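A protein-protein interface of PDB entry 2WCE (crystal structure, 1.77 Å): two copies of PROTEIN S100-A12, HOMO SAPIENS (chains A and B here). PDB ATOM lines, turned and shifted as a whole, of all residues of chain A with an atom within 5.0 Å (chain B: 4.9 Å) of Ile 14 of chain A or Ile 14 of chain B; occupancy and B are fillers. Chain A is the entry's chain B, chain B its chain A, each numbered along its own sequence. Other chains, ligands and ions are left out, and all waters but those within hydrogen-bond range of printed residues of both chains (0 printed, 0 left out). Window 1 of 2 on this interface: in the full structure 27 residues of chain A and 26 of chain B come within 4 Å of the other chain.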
ATOM      1  N   LEU A   7       0.661 -16.528  15.082  1.00  0.00           N
ATOM      2  CA  LEU A   7       0.633 -17.956  15.481  1.00  0.00           C
ATOM      3  C   LEU A   7      -0.775 -18.517  15.394  1.00  0.00           C
ATOM      4  O   LEU A   7      -1.003 -19.581  14.807  1.00  0.00           O
ATOM      5  CB  LEU A   7       1.165 -18.128  16.894  1.00  0.00           C
ATOM      6  CG  LEU A   7       1.155 -19.578  17.407  1.00  0.00           C
ATOM      7  CD1 LEU A   7       1.988 -20.491  16.518  1.00  0.00           C
ATOM      8  CD2 LEU A   7       1.601 -19.616  18.840  1.00  0.00           C
ATOM      9  N   HIS A  10      -1.961 -19.068  11.778  1.00  0.00           N
ATOM     10  CA  HIS A  10      -1.362 -20.268  11.245  1.00  0.00           C
ATOM     11  C   HIS A  10      -2.011 -21.526  11.807  1.00  0.00           C
ATOM     12  O   HIS A  10      -2.279 -22.479  11.064  1.00  0.00           O
ATOM     13  CB  HIS A  10       0.133 -20.262  11.447  1.00  0.00           C
ATOM     14  CG  HIS A  10       0.851 -19.323  10.540  1.00  0.00           C
ATOM     15  ND1 HIS A  10       1.805 -18.448  10.998  1.00  0.00           N
ATOM     16  CD2 HIS A  10       0.708 -19.069   9.219  1.00  0.00           C
ATOM     17  CE1 HIS A  10       2.274 -17.747   9.984  1.00  0.00           C
ATOM     18  NE2 HIS A  10       1.639 -18.109   8.891  1.00  0.00           N
ATOM     19  N   LEU A  11      -2.273 -21.537  13.112  1.00  0.00           N
ATOM     20  CA  LEU A  11      -2.896 -22.703  13.731  1.00  0.00           C
ATOM     21  C   LEU A  11      -4.287 -22.947  13.182  1.00  0.00           C
ATOM     22  O   LEU A  11      -4.677 -24.095  12.902  1.00  0.00           O
ATOM     23  CB  LEU A  11      -2.908 -22.590  15.254  1.00  0.00           C
ATOM     24  CG  LEU A  11      -1.513 -22.685  15.881  1.00  0.00           C
ATOM     25  CD1 LEU A  11      -1.631 -22.187  17.355  1.00  0.00           C
ATOM     26  CD2 LEU A  11      -0.869 -24.082  15.811  1.00  0.00           C
ATOM     27  N   GLU A  12      -5.018 -21.864  12.936  1.00  0.00           N
ATOM     28  CA  GLU A  12      -6.371 -21.924  12.345  1.00  0.00           C
ATOM     29  C   GLU A  12      -6.310 -22.639  10.987  1.00  0.00           C
ATOM     30  O   GLU A  12      -7.108 -23.517  10.683  1.00  0.00           O
ATOM     31  CB  GLU A  12      -6.942 -20.521  12.151  1.00  0.00           C
ATOM     32  CG  GLU A  12      -8.231 -20.400  11.320  1.00  0.00           C
ATOM     33  CD  GLU A  12      -9.439 -20.951  11.997  1.00  0.00           C
ATOM     34  OE1 GLU A  12     -10.499 -21.119  11.288  1.00  0.00           O
ATOM     35  OE2 GLU A  12      -9.355 -21.171  13.241  1.00  0.00           O
ATOM     36  N   GLY A  13      -5.328 -22.269  10.193  1.00  0.00           N
ATOM     37  CA  GLY A  13      -5.118 -22.861   8.885  1.00  0.00           C
ATOM     38  C   GLY A  13      -4.912 -24.371   8.986  1.00  0.00           C
ATOM     39  O   GLY A  13      -5.500 -25.146   8.216  1.00  0.00           O
ATOM     40  N   ILE A  14      -4.091 -24.760   9.941  1.00  0.00           N
ATOM     41  CA  ILE A  14      -3.719 -26.165  10.147  1.00  0.00           C
ATOM     42  C   ILE A  14      -4.923 -26.967  10.644  1.00  0.00           C
ATOM     43  O   ILE A  14      -5.192 -28.090  10.165  1.00  0.00           O
ATOM     44  CB  ILE A  14      -2.531 -26.299  11.050  1.00  0.00           C
ATOM     45  CG1 ILE A  14      -1.288 -25.722  10.368  1.00  0.00           C
ATOM     46  CG2 ILE A  14      -2.280 -27.773  11.345  1.00  0.00           C
ATOM     47  CD1 ILE A  14      -0.103 -25.729  11.223  1.00  0.00           C
ATOM     48  N   VAL A  15      -5.696 -26.364  11.555  1.00  0.00           N
ATOM     49  CA  VAL A  15      -6.910 -27.009  12.041  1.00  0.00           C
ATOM     50  C   VAL A  15      -7.895 -27.285  10.919  1.00  0.00           C
ATOM     51  O   VAL A  15      -8.555 -28.343  10.861  1.00  0.00           O
ATOM     52  CB  VAL A  15      -7.577 -26.130  13.132  1.00  0.00           C
ATOM     53  CG1 VAL A  15      -9.033 -26.564  13.314  1.00  0.00           C
ATOM     54  CG2 VAL A  15      -6.756 -26.209  14.420  1.00  0.00           C
ATOM     55  N   ASN A  16      -8.016 -26.326  10.027  1.00  0.00           N
ATOM     56  CA  ASN A  16      -8.944 -26.460   8.948  1.00  0.00           C
ATOM     57  C   ASN A  16      -8.521 -27.573   7.977  1.00  0.00           C
ATOM     58  O   ASN A  16      -9.366 -28.336   7.510  1.00  0.00           O
ATOM     59  CB  ASN A  16      -9.131 -25.123   8.272  1.00  0.00           C
ATOM     60  CG  ASN A  16      -9.907 -24.151   9.159  1.00  0.00           C
ATOM     61  OD1 ASN A  16     -10.723 -24.570  10.033  1.00  0.00           O
ATOM     62  ND2 ASN A  16      -9.682 -22.873   8.954  1.00  0.00           N
ATOM     63  N   ILE A  17      -7.219 -27.692   7.731  1.00  0.00           N
ATOM     64  CA  ILE A  17      -6.728 -28.621   6.751  1.00  0.00           C
ATOM     65  C   ILE A  17      -6.923 -30.035   7.335  1.00  0.00           C
ATOM     66  O   ILE A  17      -7.386 -30.969   6.634  1.00  0.00           O
ATOM     67  CB  ILE A  17      -5.222 -28.349   6.447  1.00  0.00           C
ATOM     68  CG1 ILE A  17      -5.075 -27.121   5.554  1.00  0.00           C
ATOM     69  CG2 ILE A  17      -4.626 -29.619   5.812  1.00  0.00           C
ATOM     70  CD1 ILE A  17      -3.718 -26.470   5.547  1.00  0.00           C
ATOM     71  N   PHE A  18      -6.586 -30.215   8.622  1.00  0.00           N
ATOM     72  CA  PHE A  18      -6.792 -31.502   9.275  1.00  0.00           C
ATOM     73  C   PHE A  18      -8.250 -31.952   9.075  1.00  0.00           C
ATOM     74  O   PHE A  18      -8.530 -33.096   8.705  1.00  0.00           O
ATOM     75  CB  PHE A  18      -6.463 -31.471  10.779  1.00  0.00           C
ATOM     76  CG  PHE A  18      -6.817 -32.749  11.503  1.00  0.00           C
ATOM     77  CD1 PHE A  18      -5.990 -33.865  11.413  1.00  0.00           C
ATOM     78  CD2 PHE A  18      -8.019 -32.877  12.169  1.00  0.00           C
ATOM     79  CE1 PHE A  18      -6.330 -35.043  12.071  1.00  0.00           C
ATOM     80  CE2 PHE A  18      -8.354 -34.045  12.805  1.00  0.00           C
ATOM     81  CZ  PHE A  18      -7.527 -35.130  12.757  1.00  0.00           C
ATOM     82  N   PHE A  74      -6.498 -34.954  16.053  1.00  0.00           N
ATOM     83  CA  PHE A  74      -5.693 -33.797  15.719  1.00  0.00           C
ATOM     84  C   PHE A  74      -4.349 -33.777  16.459  1.00  0.00           C
ATOM     85  O   PHE A  74      -3.310 -33.468  15.845  1.00  0.00           O
ATOM     86  CB  PHE A  74      -6.444 -32.535  16.047  1.00  0.00           C
ATOM     87  CG  PHE A  74      -5.678 -31.293  15.751  1.00  0.00           C
ATOM     88  CD1 PHE A  74      -5.554 -30.840  14.447  1.00  0.00           C
ATOM     89  CD2 PHE A  74      -5.108 -30.555  16.768  1.00  0.00           C
ATOM     90  CE1 PHE A  74      -4.873 -29.751  14.151  1.00  0.00           C
ATOM     91  CE2 PHE A  74      -4.394 -29.413  16.466  1.00  0.00           C
ATOM     92  CZ  PHE A  74      -4.282 -28.985  15.172  1.00  0.00           C
ATOM     93  N   PHE A  77      -1.933 -36.166  14.836  1.00  0.00           N
ATOM     94  CA  PHE A  77      -1.564 -35.634  13.570  1.00  0.00           C
ATOM     95  C   PHE A  77      -0.447 -34.597  13.754  1.00  0.00           C
ATOM     96  O   PHE A  77       0.591 -34.655  13.074  1.00  0.00           O
ATOM     97  CB  PHE A  77      -2.813 -35.029  12.894  1.00  0.00           C
ATOM     98  CG  PHE A  77      -2.539 -33.945  11.948  1.00  0.00           C
ATOM     99  CD1 PHE A  77      -2.086 -34.201  10.679  1.00  0.00           C
ATOM    100  CD2 PHE A  77      -2.778 -32.619  12.307  1.00  0.00           C
ATOM    101  CE1 PHE A  77      -1.885 -33.161   9.789  1.00  0.00           C
ATOM    102  CE2 PHE A  77      -2.562 -31.572  11.431  1.00  0.00           C
ATOM    103  CZ  PHE A  77      -2.098 -31.831  10.167  1.00  0.00           C
ATOM    104  N   ILE A  78      -0.634 -33.731  14.743  1.00  0.00           N
ATOM    105  CA  ILE A  78       0.348 -32.673  15.017  1.00  0.00           C
ATOM    106  C   ILE A  78       1.701 -33.235  15.380  1.00  0.00           C
ATOM    107  O   ILE A  78       2.752 -32.748  14.908  1.00  0.00           O
ATOM    108  CB  ILE A  78      -0.166 -31.745  16.167  1.00  0.00           C
ATOM    109  CG1 ILE A  78      -1.145 -30.786  15.561  1.00  0.00           C
ATOM    110  CG2 ILE A  78       1.000 -31.025  16.793  1.00  0.00           C
ATOM    111  CD1 ILE A  78      -0.504 -29.789  14.556  1.00  0.00           C
ATOM    112  N   LEU B   7      -0.416 -26.102   4.090  1.00  0.00           N
ATOM    113  CA  LEU B   7       0.040 -26.672   5.353  1.00  0.00           C
ATOM    114  C   LEU B   7       1.489 -26.297   5.605  1.00  0.00           C
ATOM    115  O   LEU B   7       1.847 -25.870   6.706  1.00  0.00           O
ATOM    116  CB  LEU B   7      -0.103 -28.197   5.368  1.00  0.00           C
ATOM    117  CG  LEU B   7       0.350 -28.912   6.634  1.00  0.00           C
ATOM    118  CD1 LEU B   7      -0.395 -28.322   7.867  1.00  0.00           C
ATOM    119  CD2 LEU B   7       0.219 -30.446   6.541  1.00  0.00           C
ATOM    120  N   HIS B  10       1.951 -22.620   6.542  1.00  0.00           N
ATOM    121  CA  HIS B  10       1.572 -22.416   7.915  1.00  0.00           C
ATOM    122  C   HIS B  10       2.640 -22.928   8.898  1.00  0.00           C
ATOM    123  O   HIS B  10       2.980 -22.262   9.866  1.00  0.00           O
ATOM    124  CB  HIS B  10       0.217 -23.050   8.199  1.00  0.00           C
ATOM    125  CG  HIS B  10      -0.922 -22.288   7.629  1.00  0.00           C
ATOM    126  ND1 HIS B  10      -1.938 -22.877   6.917  1.00  0.00           N
ATOM    127  CD2 HIS B  10      -1.201 -20.967   7.660  1.00  0.00           C
ATOM    128  CE1 HIS B  10      -2.801 -21.945   6.548  1.00  0.00           C
ATOM    129  NE2 HIS B  10      -2.376 -20.781   6.984  1.00  0.00           N
ATOM    130  N   LEU B  11       3.155 -24.129   8.655  1.00  0.00           N
ATOM    131  CA  LEU B  11       4.210 -24.652   9.467  1.00  0.00           C
ATOM    132  C   LEU B  11       5.469 -23.795   9.447  1.00  0.00           C
ATOM    133  O   LEU B  11       6.148 -23.630  10.491  1.00  0.00           O
ATOM    134  CB  LEU B  11       4.517 -26.087   9.064  1.00  0.00           C
ATOM    135  CG  LEU B  11       3.397 -27.089   9.319  1.00  0.00           C
ATOM    136  CD1 LEU B  11       3.790 -28.344   8.623  1.00  0.00           C
ATOM    137  CD2 LEU B  11       3.210 -27.356  10.842  1.00  0.00           C
ATOM    138  N   GLU B  12       5.781 -23.242   8.271  1.00  0.00           N
ATOM    139  CA  GLU B  12       6.928 -22.331   8.093  1.00  0.00           C
ATOM    140  C   GLU B  12       6.779 -21.169   9.058  1.00  0.00           C
ATOM    141  O   GLU B  12       7.706 -20.818   9.814  1.00  0.00           O
ATOM    142  CB  GLU B  12       7.001 -21.821   6.622  1.00  0.00           C
ATOM    143  CG  GLU B  12       7.969 -20.642   6.393  1.00  0.00           C
ATOM    144  CD  GLU B  12       7.916 -20.032   4.987  1.00  0.00           C
ATOM    145  OE1 GLU B  12       7.005 -20.341   4.194  1.00  0.00           O
ATOM    146  OE2 GLU B  12       8.794 -19.199   4.675  1.00  0.00           O
ATOM    147  N   GLY B  13       5.572 -20.620   9.096  1.00  0.00           N
ATOM    148  CA  GLY B  13       5.296 -19.462   9.955  1.00  0.00           C
ATOM    149  C   GLY B  13       5.438 -19.794  11.447  1.00  0.00           C
ATOM    150  O   GLY B  13       5.984 -18.978  12.239  1.00  0.00           O
ATOM    151  N   ILE B  14       4.941 -20.966  11.843  1.00  0.00           N
ATOM    152  CA  ILE B  14       5.043 -21.422  13.211  1.00  0.00           C
ATOM    153  C   ILE B  14       6.487 -21.704  13.629  1.00  0.00           C
ATOM    154  O   ILE B  14       6.908 -21.288  14.725  1.00  0.00           O
ATOM    155  CB  ILE B  14       4.116 -22.618  13.478  1.00  0.00           C
ATOM    156  CG1 ILE B  14       2.673 -22.228  13.123  1.00  0.00           C
ATOM    157  CG2 ILE B  14       4.259 -23.070  14.947  1.00  0.00           C
ATOM    158  CD1 ILE B  14       1.690 -23.411  13.027  1.00  0.00           C
ATOM    159  N   VAL B  15       7.225 -22.353  12.756  1.00  0.00           N
ATOM    160  CA  VAL B  15       8.670 -22.577  12.969  1.00  0.00           C
ATOM    161  C   VAL B  15       9.395 -21.268  13.198  1.00  0.00           C
ATOM    162  O   VAL B  15      10.240 -21.153  14.127  1.00  0.00           O
ATOM    163  CB  VAL B  15       9.266 -23.377  11.813  1.00  0.00           C
ATOM    164  CG1 VAL B  15      10.789 -23.331  11.831  1.00  0.00           C
ATOM    165  CG2 VAL B  15       8.799 -24.856  11.921  1.00  0.00           C
ATOM    166  N   ASN B  16       9.103 -20.274  12.377  1.00  0.00           N
ATOM    167  CA  ASN B  16       9.770 -18.997  12.512  1.00  0.00           C
ATOM    168  C   ASN B  16       9.454 -18.345  13.892  1.00  0.00           C
ATOM    169  O   ASN B  16      10.346 -17.792  14.547  1.00  0.00           O
ATOM    170  CB  ASN B  16       9.365 -18.056  11.370  1.00  0.00           C
ATOM    171  CG  ASN B  16      10.130 -16.800  11.392  1.00  0.00           C
ATOM    172  OD1 ASN B  16       9.869 -15.915  12.233  1.00  0.00           O
ATOM    173  ND2 ASN B  16      11.124 -16.685  10.491  1.00  0.00           N
ATOM    174  N   ILE B  17       8.184 -18.380  14.293  1.00  0.00           N
ATOM    175  CA  ILE B  17       7.761 -17.753  15.537  1.00  0.00           C
ATOM    176  C   ILE B  17       8.432 -18.454  16.707  1.00  0.00           C
ATOM    177  O   ILE B  17       8.932 -17.806  17.624  1.00  0.00           O
ATOM    178  CB  ILE B  17       6.231 -17.775  15.699  1.00  0.00           C
ATOM    179  CG1 ILE B  17       5.569 -16.770  14.735  1.00  0.00           C
ATOM    180  CG2 ILE B  17       5.859 -17.463  17.172  1.00  0.00           C
ATOM    181  CD1 ILE B  17       4.124 -17.118  14.399  1.00  0.00           C
ATOM    182  N   PHE B  18       8.446 -19.780  16.681  1.00  0.00           N
ATOM    183  CA  PHE B  18       9.081 -20.547  17.740  1.00  0.00           C
ATOM    184  C   PHE B  18      10.547 -20.100  17.875  1.00  0.00           C
ATOM    185  O   PHE B  18      11.032 -19.883  18.966  1.00  0.00           O
ATOM    186  CB  PHE B  18       9.009 -22.037  17.462  1.00  0.00           C
ATOM    187  CG  PHE B  18       9.830 -22.863  18.407  1.00  0.00           C
ATOM    188  CD1 PHE B  18       9.332 -23.209  19.643  1.00  0.00           C
ATOM    189  CD2 PHE B  18      11.147 -23.226  18.087  1.00  0.00           C
ATOM    190  CE1 PHE B  18      10.110 -23.993  20.525  1.00  0.00           C
ATOM    191  CE2 PHE B  18      11.909 -23.962  18.976  1.00  0.00           C
ATOM    192  CZ  PHE B  18      11.418 -24.329  20.174  1.00  0.00           C
ATOM    193  N   PHE B  74      10.837 -27.790  19.667  1.00  0.00           N
ATOM    194  CA  PHE B  74       9.669 -27.532  18.857  1.00  0.00           C
ATOM    195  C   PHE B  74       8.571 -28.567  19.031  1.00  0.00           C
ATOM    196  O   PHE B  74       7.369 -28.231  19.125  1.00  0.00           O
ATOM    197  CB  PHE B  74      10.074 -27.409  17.385  1.00  0.00           C
ATOM    198  CG  PHE B  74       8.939 -27.031  16.496  1.00  0.00           C
ATOM    199  CD1 PHE B  74       8.600 -25.703  16.322  1.00  0.00           C
ATOM    200  CD2 PHE B  74       8.245 -27.994  15.800  1.00  0.00           C
ATOM    201  CE1 PHE B  74       7.547 -25.332  15.508  1.00  0.00           C
ATOM    202  CE2 PHE B  74       7.168 -27.635  15.013  1.00  0.00           C
ATOM    203  CZ  PHE B  74       6.834 -26.300  14.856  1.00  0.00           C
ATOM    204  N   PHE B  77       6.714 -27.952  22.282  1.00  0.00           N
ATOM    205  CA  PHE B  77       5.975 -26.697  22.080  1.00  0.00           C
ATOM    206  C   PHE B  77       4.679 -26.943  21.305  1.00  0.00           C
ATOM    207  O   PHE B  77       3.572 -26.583  21.768  1.00  0.00           O
ATOM    208  CB  PHE B  77       6.856 -25.698  21.303  1.00  0.00           C
ATOM    209  CG  PHE B  77       6.123 -24.681  20.539  1.00  0.00           C
ATOM    210  CD1 PHE B  77       5.499 -23.613  21.176  1.00  0.00           C
ATOM    211  CD2 PHE B  77       6.087 -24.714  19.154  1.00  0.00           C
ATOM    212  CE1 PHE B  77       4.846 -22.641  20.431  1.00  0.00           C
ATOM    213  CE2 PHE B  77       5.426 -23.763  18.431  1.00  0.00           C
ATOM    214  CZ  PHE B  77       4.800 -22.722  19.081  1.00  0.00           C
ATOM    215  N   ILE B  78       4.786 -27.665  20.193  1.00  0.00           N
ATOM    216  CA  ILE B  78       3.595 -27.764  19.316  1.00  0.00           C
ATOM    217  C   ILE B  78       2.575 -28.709  19.954  1.00  0.00           C
ATOM    218  O   ILE B  78       1.366 -28.521  19.807  1.00  0.00           O
ATOM    219  CB  ILE B  78       4.019 -28.015  17.803  1.00  0.00           C
ATOM    220  CG1 ILE B  78       2.910 -27.572  16.815  1.00  0.00           C
ATOM    221  CG2 ILE B  78       4.379 -29.382  17.625  1.00  0.00           C
ATOM    222  CD1 ILE B  78       2.603 -26.105  16.807  1.00  0.00           C
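Printed residues of chain B within 4 Å of Ile 14 of chain A: Leu 7, His 10, Leu 11 and Ile 14. Ile 14 of chain B touches just these residues of chain A: Leu 7, His 10, Leu 11 and Ile 14. Of the printed residues of chain B, Gly 13 of chain A touches His 10. Of the printed residues of chain B, Leu 7 of chain A touches Ile 14 (3.8 Å) and Ile 17 (3.6 Å). Printed residues of chain A within 4 Å of Leu 7 of chain B: Ile 14 and Ile 17. Printed residues of chain B within 4 Å of Ile 78 of chain A: Ile 78. Of the printed residues of chain A, Ile 17 of chain B touches Leu 7 (3.6 Å). The nearest printed residue of chain B that does not touch Ile 14 of chain A is Ile 78 of chain B (6.2 Å). The nearest printed residue of chain A that does not touch Ile 14 of chain B is Glu 12 of chain A (6.9 Å). The nearest printed residue of chain A that does not touch Gly 13 of chain B is Leu 7 of chain A (6.0 Å).
Leu 7 of chain A touches Ile 14 of chain B, and with the chains exchanged Ile 14 of chain A touches Leu 7 of chain B. His 10 of chain A touches Gly 13 of chain B, and with the chains exchanged Gly 13 of chain A touches His 10 of chain B. His 10 of chain A touches Ile 14 of chain B, and with the chains exchanged Ile 14 of chain A touches His 10 of chain B. Leu 11 of chain A touches Ile 14 of chain B, and with the chains exchanged Ile 14 of chain A touches Leu 11 of chain B. Positions printed for both chains: 7, 10, 11, 12, 13, 14, 15, 16, 17, 18, 74, 77 and 78. Of the 13 pairs that touch across the chains among the printed residues, 13 have their exchanged pair printed and touching as well.
Hydrophobic or aromatic side chains of chain B within 4 Å of the printed part of chain A: Leu 7, His 10, Leu 11, Ile 14, Ile 17 and Ile 78. Of the 13 printed residues of chain A, 7 touch a printed residue of chain B. Printed residues of chain A that touch a printed residue of chain B: Leu 7, His 10, Leu 11, Gly 13, Ile 14, Ile 17 and Ile 78. Hydrophobic or aromatic side chains of chain A within 4 Å of the printed part of chain B: Leu 7, His 10, Leu 11, Ile 14, Ile 17 and Ile 78. Among the printed residues, 13 pairs touch across the chains.
Leu 7 of chain A touches Ile 14 of chain B. N of Leu 7 of chain A touches CD1 of Ile 17 of chain B, 3.6 Å away. His 10 of chain B touches His 10 of chain A. Gly 13 of chain B touches His 10 of chain A (CA to CE1, 3.5 Å). His 10 of chain A touches Ile 14 of chain B. CD1 of Ile 14 of chain B touches CD2 of Leu 11 of chain A, 3.8 Å away. CA of Gly 13 of chain A touches CE1 of His 10 of chain B (3.4 Å). CG1 of Ile 14 of chain A touches CD1 of Leu 7 of chain B (3.7 Å). Ile 14 of chain B touches Ile 14 of chain A (CD1 to CD1, 3.4 Å). Leu 7 of chain B touches Ile 17 of chain A (N to CD1, 3.6 Å).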
